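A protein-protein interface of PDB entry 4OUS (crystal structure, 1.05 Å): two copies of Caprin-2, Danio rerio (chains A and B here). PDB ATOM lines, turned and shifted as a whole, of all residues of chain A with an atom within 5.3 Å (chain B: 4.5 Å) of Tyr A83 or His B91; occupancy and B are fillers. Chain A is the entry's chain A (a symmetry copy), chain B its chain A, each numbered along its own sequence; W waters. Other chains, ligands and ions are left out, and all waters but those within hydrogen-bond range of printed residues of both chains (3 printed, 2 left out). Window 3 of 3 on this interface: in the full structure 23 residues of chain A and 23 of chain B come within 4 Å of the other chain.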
ATOM      1  N   PRO A  67      21.243 -38.527   6.079  1.00  0.00           N
ATOM      2  CA  PRO A  67      20.947 -37.147   5.699  1.00  0.00           C
ATOM      3  C   PRO A  67      19.462 -36.936   5.468  1.00  0.00           C
ATOM      4  O   PRO A  67      18.732 -37.878   5.143  1.00  0.00           O
ATOM      5  CB  PRO A  67      21.724 -36.972   4.396  1.00  0.00           C
ATOM      6  CG  PRO A  67      21.774 -38.359   3.825  1.00  0.00           C
ATOM      7  CD  PRO A  67      21.985 -39.236   5.024  1.00  0.00           C
ATOM      8  N   LEU A  68      19.031 -35.692   5.625  1.00  0.00           N
ATOM      9  CA  LEU A  68      17.652 -35.305   5.383  1.00  0.00           C
ATOM     10  C   LEU A  68      17.520 -34.636   4.021  1.00  0.00           C
ATOM     11  O   LEU A  68      18.201 -33.646   3.744  1.00  0.00           O
ATOM     12  CB  LEU A  68      17.160 -34.370   6.485  1.00  0.00           C
ATOM     13  CG  LEU A  68      15.701 -33.937   6.372  1.00  0.00           C
ATOM     14  CD1 LEU A  68      14.778 -35.121   6.590  1.00  0.00           C
ATOM     15  CD2 LEU A  68      15.362 -32.814   7.342  1.00  0.00           C
ATOM     16  N   TYR A  69      16.655 -35.186   3.175  1.00  0.00           N
ATOM     17  CA  TYR A  69      16.308 -34.612   1.878  1.00  0.00           C
ATOM     18  C   TYR A  69      14.806 -34.387   1.837  1.00  0.00           C
ATOM     19  O   TYR A  69      14.041 -35.345   2.011  1.00  0.00           O
ATOM     20  CB  TYR A  69      16.682 -35.549   0.734  1.00  0.00           C
ATOM     21  CG  TYR A  69      18.142 -35.720   0.405  1.00  0.00           C
ATOM     22  CD1 TYR A  69      18.694 -35.067  -0.695  1.00  0.00           C
ATOM     23  CD2 TYR A  69      18.963 -36.570   1.144  1.00  0.00           C
ATOM     24  CE1 TYR A  69      20.017 -35.238  -1.038  1.00  0.00           C
ATOM     25  CE2 TYR A  69      20.292 -36.750   0.801  1.00  0.00           C
ATOM     26  CZ  TYR A  69      20.812 -36.080  -0.290  1.00  0.00           C
ATOM     27  OH  TYR A  69      22.137 -36.243  -0.638  1.00  0.00           O
ATOM     28  N   ILE A  70      14.395 -33.149   1.587  1.00  0.00           N
ATOM     29  CA  ILE A  70      12.992 -32.772   1.479  1.00  0.00           C
ATOM     30  C   ILE A  70      12.728 -32.205   0.093  1.00  0.00           C
ATOM     31  O   ILE A  70      13.524 -31.400  -0.402  1.00  0.00           O
ATOM     32  CB  ILE A  70      12.612 -31.693   2.523  1.00  0.00           C
ATOM     33  CG1 ILE A  70      12.933 -32.138   3.950  1.00  0.00           C
ATOM     34  CG2 ILE A  70      11.154 -31.290   2.390  1.00  0.00           C
ATOM     35  CD1 ILE A  70      12.095 -33.290   4.437  1.00  0.00           C
ATOM     36  N   SER A  81      13.980 -28.143  -3.447  1.00  0.00           N
ATOM     37  CA  SER A  81      14.412 -29.158  -2.500  1.00  0.00           C
ATOM     38  C   SER A  81      15.284 -28.570  -1.403  1.00  0.00           C
ATOM     39  O   SER A  81      15.781 -27.446  -1.513  1.00  0.00           O
ATOM     40  CB  SER A  81      15.179 -30.269  -3.219  1.00  0.00           C
ATOM     41  OG  SER A  81      14.398 -30.845  -4.255  1.00  0.00           O
ATOM     42  N   ALA A  82      15.464 -29.346  -0.341  1.00  0.00           N
ATOM     43  CA  ALA A  82      16.322 -28.939   0.759  1.00  0.00           C
ATOM     44  C   ALA A  82      17.084 -30.138   1.290  1.00  0.00           C
ATOM     45  O   ALA A  82      16.599 -31.266   1.248  1.00  0.00           O
ATOM     46  CB  ALA A  82      15.510 -28.291   1.871  1.00  0.00           C
ATOM     47  N   TYR A  83      18.276 -29.862   1.802  1.00  0.00           N
ATOM     48  CA  TYR A  83      19.184 -30.869   2.336  1.00  0.00           C
ATOM     49  C   TYR A  83      19.662 -30.437   3.701  1.00  0.00           C
ATOM     50  O   TYR A  83      19.937 -29.249   3.905  1.00  0.00           O
ATOM     51  CB  TYR A  83      20.386 -31.041   1.407  1.00  0.00           C
ATOM     52  CG  TYR A  83      21.500 -31.928   1.931  1.00  0.00           C
ATOM     53  CD1 TYR A  83      21.511 -33.284   1.653  1.00  0.00           C
ATOM     54  CD2 TYR A  83      22.545 -31.405   2.688  1.00  0.00           C
ATOM     55  CE1 TYR A  83      22.530 -34.104   2.107  1.00  0.00           C
ATOM     56  CE2 TYR A  83      23.572 -32.222   3.155  1.00  0.00           C
ATOM     57  CZ  TYR A  83      23.559 -33.573   2.858  1.00  0.00           C
ATOM     58  OH  TYR A  83      24.564 -34.413   3.295  1.00  0.00           O
ATOM     59  N   ALA A  84      19.811 -31.382   4.621  1.00  0.00           N
ATOM     60  CA  ALA A  84      20.495 -31.068   5.867  1.00  0.00           C
ATOM     61  C   ALA A  84      21.173 -32.304   6.412  1.00  0.00           C
ATOM     62  O   ALA A  84      20.603 -33.394   6.397  1.00  0.00           O
ATOM     63  CB  ALA A  84      19.530 -30.491   6.892  1.00  0.00           C
ATOM     64  N   ASN A  85      22.383 -32.125   6.915  1.00  0.00           N
ATOM     65  CA  ASN A  85      23.090 -33.225   7.523  1.00  0.00           C
ATOM     66  C   ASN A  85      24.182 -32.701   8.420  1.00  0.00           C
ATOM     67  O   ASN A  85      24.773 -31.662   8.142  1.00  0.00           O
ATOM     68  CB  ASN A  85      23.672 -34.134   6.451  1.00  0.00           C
ATOM     69  CG  ASN A  85      24.101 -35.464   6.997  1.00  0.00           C
ATOM     70  OD1 ASN A  85      23.411 -36.052   7.828  1.00  0.00           O
ATOM     71  ND2 ASN A  85      25.248 -35.953   6.539  1.00  0.00           N
ATOM     72  N   THR A  93      18.653 -28.517   9.985  1.00  0.00           N
ATOM     73  CA  THR A  93      17.391 -28.046   9.435  1.00  0.00           C
ATOM     74  C   THR A  93      17.446 -27.949   7.919  1.00  0.00           C
ATOM     75  O   THR A  93      18.344 -27.306   7.363  1.00  0.00           O
ATOM     76  CB  THR A  93      17.018 -26.680  10.031  1.00  0.00           C
ATOM     77  OG1 THR A  93      17.078 -26.766  11.459  1.00  0.00           O
ATOM     78  CG2 THR A  93      15.624 -26.248   9.605  1.00  0.00           C
ATOM     79  N   ALA A  94      16.482 -28.588   7.264  1.00  0.00           N
ATOM     80  CA  ALA A  94      16.293 -28.504   5.821  1.00  0.00           C
ATOM     81  C   ALA A  94      15.159 -27.532   5.544  1.00  0.00           C
ATOM     82  O   ALA A  94      14.021 -27.761   5.986  1.00  0.00           O
ATOM     83  CB  ALA A  94      15.985 -29.878   5.240  1.00  0.00           C
ATOM     84  N   LEU B  60      22.480 -23.535  -1.138  1.00  0.00           N
ATOM     85  CA  LEU B  60      23.219 -24.709  -0.689  1.00  0.00           C
ATOM     86  C   LEU B  60      24.667 -24.606  -1.152  1.00  0.00           C
ATOM     87  O   LEU B  60      24.918 -24.361  -2.337  1.00  0.00           O
ATOM     88  CB  LEU B  60      22.578 -25.988  -1.235  1.00  0.00           C
ATOM     89  CG  LEU B  60      23.091 -27.298  -0.636  1.00  0.00           C
ATOM     90  CD1 LEU B  60      22.570 -27.475   0.783  1.00  0.00           C
ATOM     91  CD2 LEU B  60      22.714 -28.490  -1.508  1.00  0.00           C
ATOM     92  N   LYS B  61      25.617 -24.790  -0.238  1.00  0.00           N
ATOM     93  CA  LYS B  61      27.029 -24.720  -0.607  1.00  0.00           C
ATOM     94  C   LYS B  61      27.556 -26.040  -1.136  1.00  0.00           C
ATOM     95  O   LYS B  61      27.024 -27.105  -0.814  1.00  0.00           O
ATOM     96  CB  LYS B  61      27.885 -24.279   0.582  1.00  0.00           C
ATOM     97  CG  LYS B  61      28.073 -25.331   1.672  1.00  0.00           C
ATOM     98  CD  LYS B  61      28.774 -24.773   2.920  1.00  0.00           C
ATOM     99  CE  LYS B  61      30.174 -24.238   2.640  1.00  0.00           C
ATOM    100  NZ  LYS B  61      31.115 -25.312   2.231  1.00  0.00           N
ATOM    101  N   LEU B  62      28.609 -25.963  -1.944  1.00  0.00           N
ATOM    102  CA  LEU B  62      29.377 -27.149  -2.293  1.00  0.00           C
ATOM    103  C   LEU B  62      30.028 -27.719  -1.041  1.00  0.00           C
ATOM    104  O   LEU B  62      30.373 -26.989  -0.100  1.00  0.00           O
ATOM    105  CB  LEU B  62      30.454 -26.838  -3.335  1.00  0.00           C
ATOM    106  CG  LEU B  62      29.988 -26.341  -4.702  1.00  0.00           C
ATOM    107  CD1 LEU B  62      31.152 -26.317  -5.683  1.00  0.00           C
ATOM    108  CD2 LEU B  62      28.871 -27.210  -5.233  1.00  0.00           C
ATOM    109  N   ALA B  63      30.220 -29.031  -1.057  1.00  0.00           N
ATOM    110  CA  ALA B  63      30.858 -29.738   0.041  1.00  0.00           C
ATOM    111  C   ALA B  63      32.373 -29.616  -0.080  1.00  0.00           C
ATOM    112  O   ALA B  63      33.075 -30.584  -0.394  1.00  0.00           O
ATOM    113  CB  ALA B  63      30.426 -31.195   0.062  1.00  0.00           C
ATOM    114  N   ASP B  90      30.539 -31.006   4.461  1.00  0.00           N
ATOM    115  CA  ASP B  90      29.256 -31.452   3.941  1.00  0.00           C
ATOM    116  C   ASP B  90      28.560 -30.246   3.323  1.00  0.00           C
ATOM    117  O   ASP B  90      29.012 -29.106   3.474  1.00  0.00           O
ATOM    118  CB  ASP B  90      28.415 -32.062   5.068  1.00  0.00           C
ATOM    119  CG  ASP B  90      27.355 -33.048   4.576  1.00  0.00           C
ATOM    120  OD1 ASP B  90      26.948 -33.001   3.398  1.00  0.00           O
ATOM    121  OD2 ASP B  90      26.919 -33.881   5.400  1.00  0.00           O
ATOM    122  N   HIS B  91      27.459 -30.490   2.627  1.00  0.00           N
ATOM    123  CA  HIS B  91      26.616 -29.395   2.192  1.00  0.00           C
ATOM    124  C   HIS B  91      25.986 -28.731   3.413  1.00  0.00           C
ATOM    125  O   HIS B  91      25.812 -29.345   4.470  1.00  0.00           O
ATOM    126  CB  HIS B  91      25.532 -29.885   1.238  1.00  0.00           C
ATOM    127  CG  HIS B  91      26.064 -30.583   0.027  1.00  0.00           C
ATOM    128  ND1 HIS B  91      26.700 -29.920  -1.000  1.00  0.00           N
ATOM    129  CD2 HIS B  91      26.047 -31.890  -0.321  1.00  0.00           C
ATOM    130  CE1 HIS B  91      27.056 -30.790  -1.928  1.00  0.00           C
ATOM    131  NE2 HIS B  91      26.672 -31.992  -1.540  1.00  0.00           N
ATOM    132  N   GLU B  92      25.674 -27.460   3.250  1.00  0.00           N
ATOM    133  CA  GLU B  92      25.080 -26.628   4.278  1.00  0.00           C
ATOM    134  C   GLU B  92      24.357 -25.501   3.570  1.00  0.00           C
ATOM    135  O   GLU B  92      24.686 -25.192   2.425  1.00  0.00           O
ATOM    136  CB  GLU B  92      26.122 -26.053   5.237  1.00  0.00           C
ATOM    137  CG  GLU B  92      26.083 -26.514   6.684  1.00  0.00           C
ATOM    138  CD  GLU B  92      24.856 -25.990   7.443  1.00  0.00           C
ATOM    139  OE1 GLU B  92      23.807 -25.687   6.831  1.00  0.00           O
ATOM    140  OE2 GLU B  92      24.993 -25.736   8.658  1.00  0.00           O
ATOM    141  N   THR B  93      23.411 -24.864   4.249  1.00  0.00           N
ATOM    142  CA  THR B  93      22.523 -23.904   3.609  1.00  0.00           C
ATOM    143  C   THR B  93      22.636 -22.530   4.246  1.00  0.00           C
ATOM    144  O   THR B  93      22.498 -22.390   5.467  1.00  0.00           O
ATOM    145  CB  THR B  93      21.067 -24.390   3.673  1.00  0.00           C
ATOM    146  OG1 THR B  93      21.003 -25.728   3.166  1.00  0.00           O
ATOM    147  CG2 THR B  93      20.145 -23.494   2.861  1.00  0.00           C
ATOM    148  N   TYR B 118      25.949 -24.994  -4.853  1.00  0.00           N
ATOM    149  CA  TYR B 118      25.448 -26.198  -5.482  1.00  0.00           C
ATOM    150  C   TYR B 118      24.215 -25.937  -6.330  1.00  0.00           C
ATOM    151  O   TYR B 118      23.210 -25.400  -5.842  1.00  0.00           O
ATOM    152  CB  TYR B 118      25.107 -27.239  -4.414  1.00  0.00           C
ATOM    153  CG  TYR B 118      24.721 -28.573  -4.997  1.00  0.00           C
ATOM    154  CD1 TYR B 118      25.695 -29.481  -5.388  1.00  0.00           C
ATOM    155  CD2 TYR B 118      23.388 -28.921  -5.178  1.00  0.00           C
ATOM    156  CE1 TYR B 118      25.353 -30.703  -5.936  1.00  0.00           C
ATOM    157  CE2 TYR B 118      23.037 -30.140  -5.725  1.00  0.00           C
ATOM    158  CZ  TYR B 118      24.020 -31.026  -6.099  1.00  0.00           C
ATOM    159  OH  TYR B 118      23.674 -32.244  -6.641  1.00  0.00           O
ATOM    160  N   TYR B 124      17.880 -26.786  -5.124  1.00  0.00           N
ATOM    161  CA  TYR B 124      18.167 -26.486  -3.722  1.00  0.00           C
ATOM    162  C   TYR B 124      18.409 -25.000  -3.473  1.00  0.00           C
ATOM    163  O   TYR B 124      18.085 -24.484  -2.400  1.00  0.00           O
ATOM    164  CB  TYR B 124      19.403 -27.253  -3.253  1.00  0.00           C
ATOM    165  CG  TYR B 124      19.243 -28.743  -3.233  1.00  0.00           C
ATOM    166  CD1 TYR B 124      18.725 -29.383  -2.121  1.00  0.00           C
ATOM    167  CD2 TYR B 124      19.625 -29.522  -4.319  1.00  0.00           C
ATOM    168  CE1 TYR B 124      18.580 -30.754  -2.083  1.00  0.00           C
ATOM    169  CE2 TYR B 124      19.482 -30.901  -4.292  1.00  0.00           C
ATOM    170  CZ  TYR B 124      18.963 -31.502  -3.166  1.00  0.00           C
ATOM    171  OH  TYR B 124      18.805 -32.865  -3.099  1.00  0.00           O
HETATM  172  O   HOH W   1      19.079 -27.088   1.551  1.00  0.00           O
HETATM  173  O   HOH W   2      21.674 -27.571   5.128  1.00  0.00           O
HETATM  174  O   HOH W   3      23.482 -29.340   6.339  1.00  0.00           O
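The backbone carbonyl oxygen of Lys B61 lies within hydrogen-bond range of a ring nitrogen (ND1) of His B91, at 2.8 Å. The backbone NH (N) of Ala A82 is in hydrogen-bond range of the backbone carbonyl oxygen (O) of Ile A70 (2.8 Å).
Of the 11 printed residues of chain A, 5 touch a printed residue of chain B. Printed residues of chain A that touch a printed residue of chain B: Tyr A69, Ser A81, Ala A82, Tyr A83 and Asn A85. Of the 10 printed residues of chain B, 4 touch a printed residue of chain A. Printed residues of chain B that touch a printed residue of chain A: Asp B90, His B91, Thr B93 and Tyr B124. Hydrophobic or aromatic side chains of chain B within 4 Å of the printed part of chain A: His B91 and Tyr B124. Among the printed residues, 8 pairs touch across the chains.
Among the printed residues, merely in contact across the chains: Tyr A69 with Tyr B124, Ser A81 with Tyr B124, Ala A82 with Tyr B124, Tyr A83 with His B91, Tyr A83 with Thr B93 and Tyr A83 with Tyr B124.
Printed residues of chain B within 4 Å of Tyr A83: Asp B90 (2.8 Å), His B91 (3.6 Å), Thr B93 (3.8 Å) and Tyr B124 (3.9 Å). His B91 touches just one residue of chain A: Tyr A83. Of the printed residues of chain A, Asp B90 touches Tyr A83 and Asn A85. Of the printed residues of chain A, Tyr B124 touches Tyr A69, Ser A81, Ala A82 and Tyr A83. Printed residues of chain B within 4 Å of Ala A82: Tyr B124 (3.7 Å). Of the printed residues of chain B, Tyr A69 touches Tyr B124. Of the printed residues of chain B, Ser A81 touches Tyr B124. Ala A84 touches none of the printed residues of chain B. Ile A70 touches none of the printed residues of chain B. The nearest printed residue of chain B that does not touch Ala A82 is Leu B60 (6.1 Å).
Position printed for both chains: 93. Of the 8 pairs that touch across the chains among the printed residues, none has its exchanged pair printed and touching as well.
OH of Tyr A83 sits at hydrogen-bond distance from OD1 of Asp B90 (2.8 Å). The side-chain carboxylate (OD2) of Asp B90 sits at hydrogen-bond distance from the side-chain amide nitrogen (ND2) of Asn A85 (2.9 Å).
Water W2 bridges the backbone carbonyl oxygen (O) of Tyr A83 (2.7 Å) and the side-chain hydroxyl (OG1) of Thr B93 (2.8 Å). Water W1 bridges the side-chain hydroxyl (OG1) of Thr B93 (2.9 Å) and the backbone NH (N) of Tyr A83 (2.9 Å). Water W3 bridges O of His B91 (3.0 Å) and N of Asn A85 (3.0 Å).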
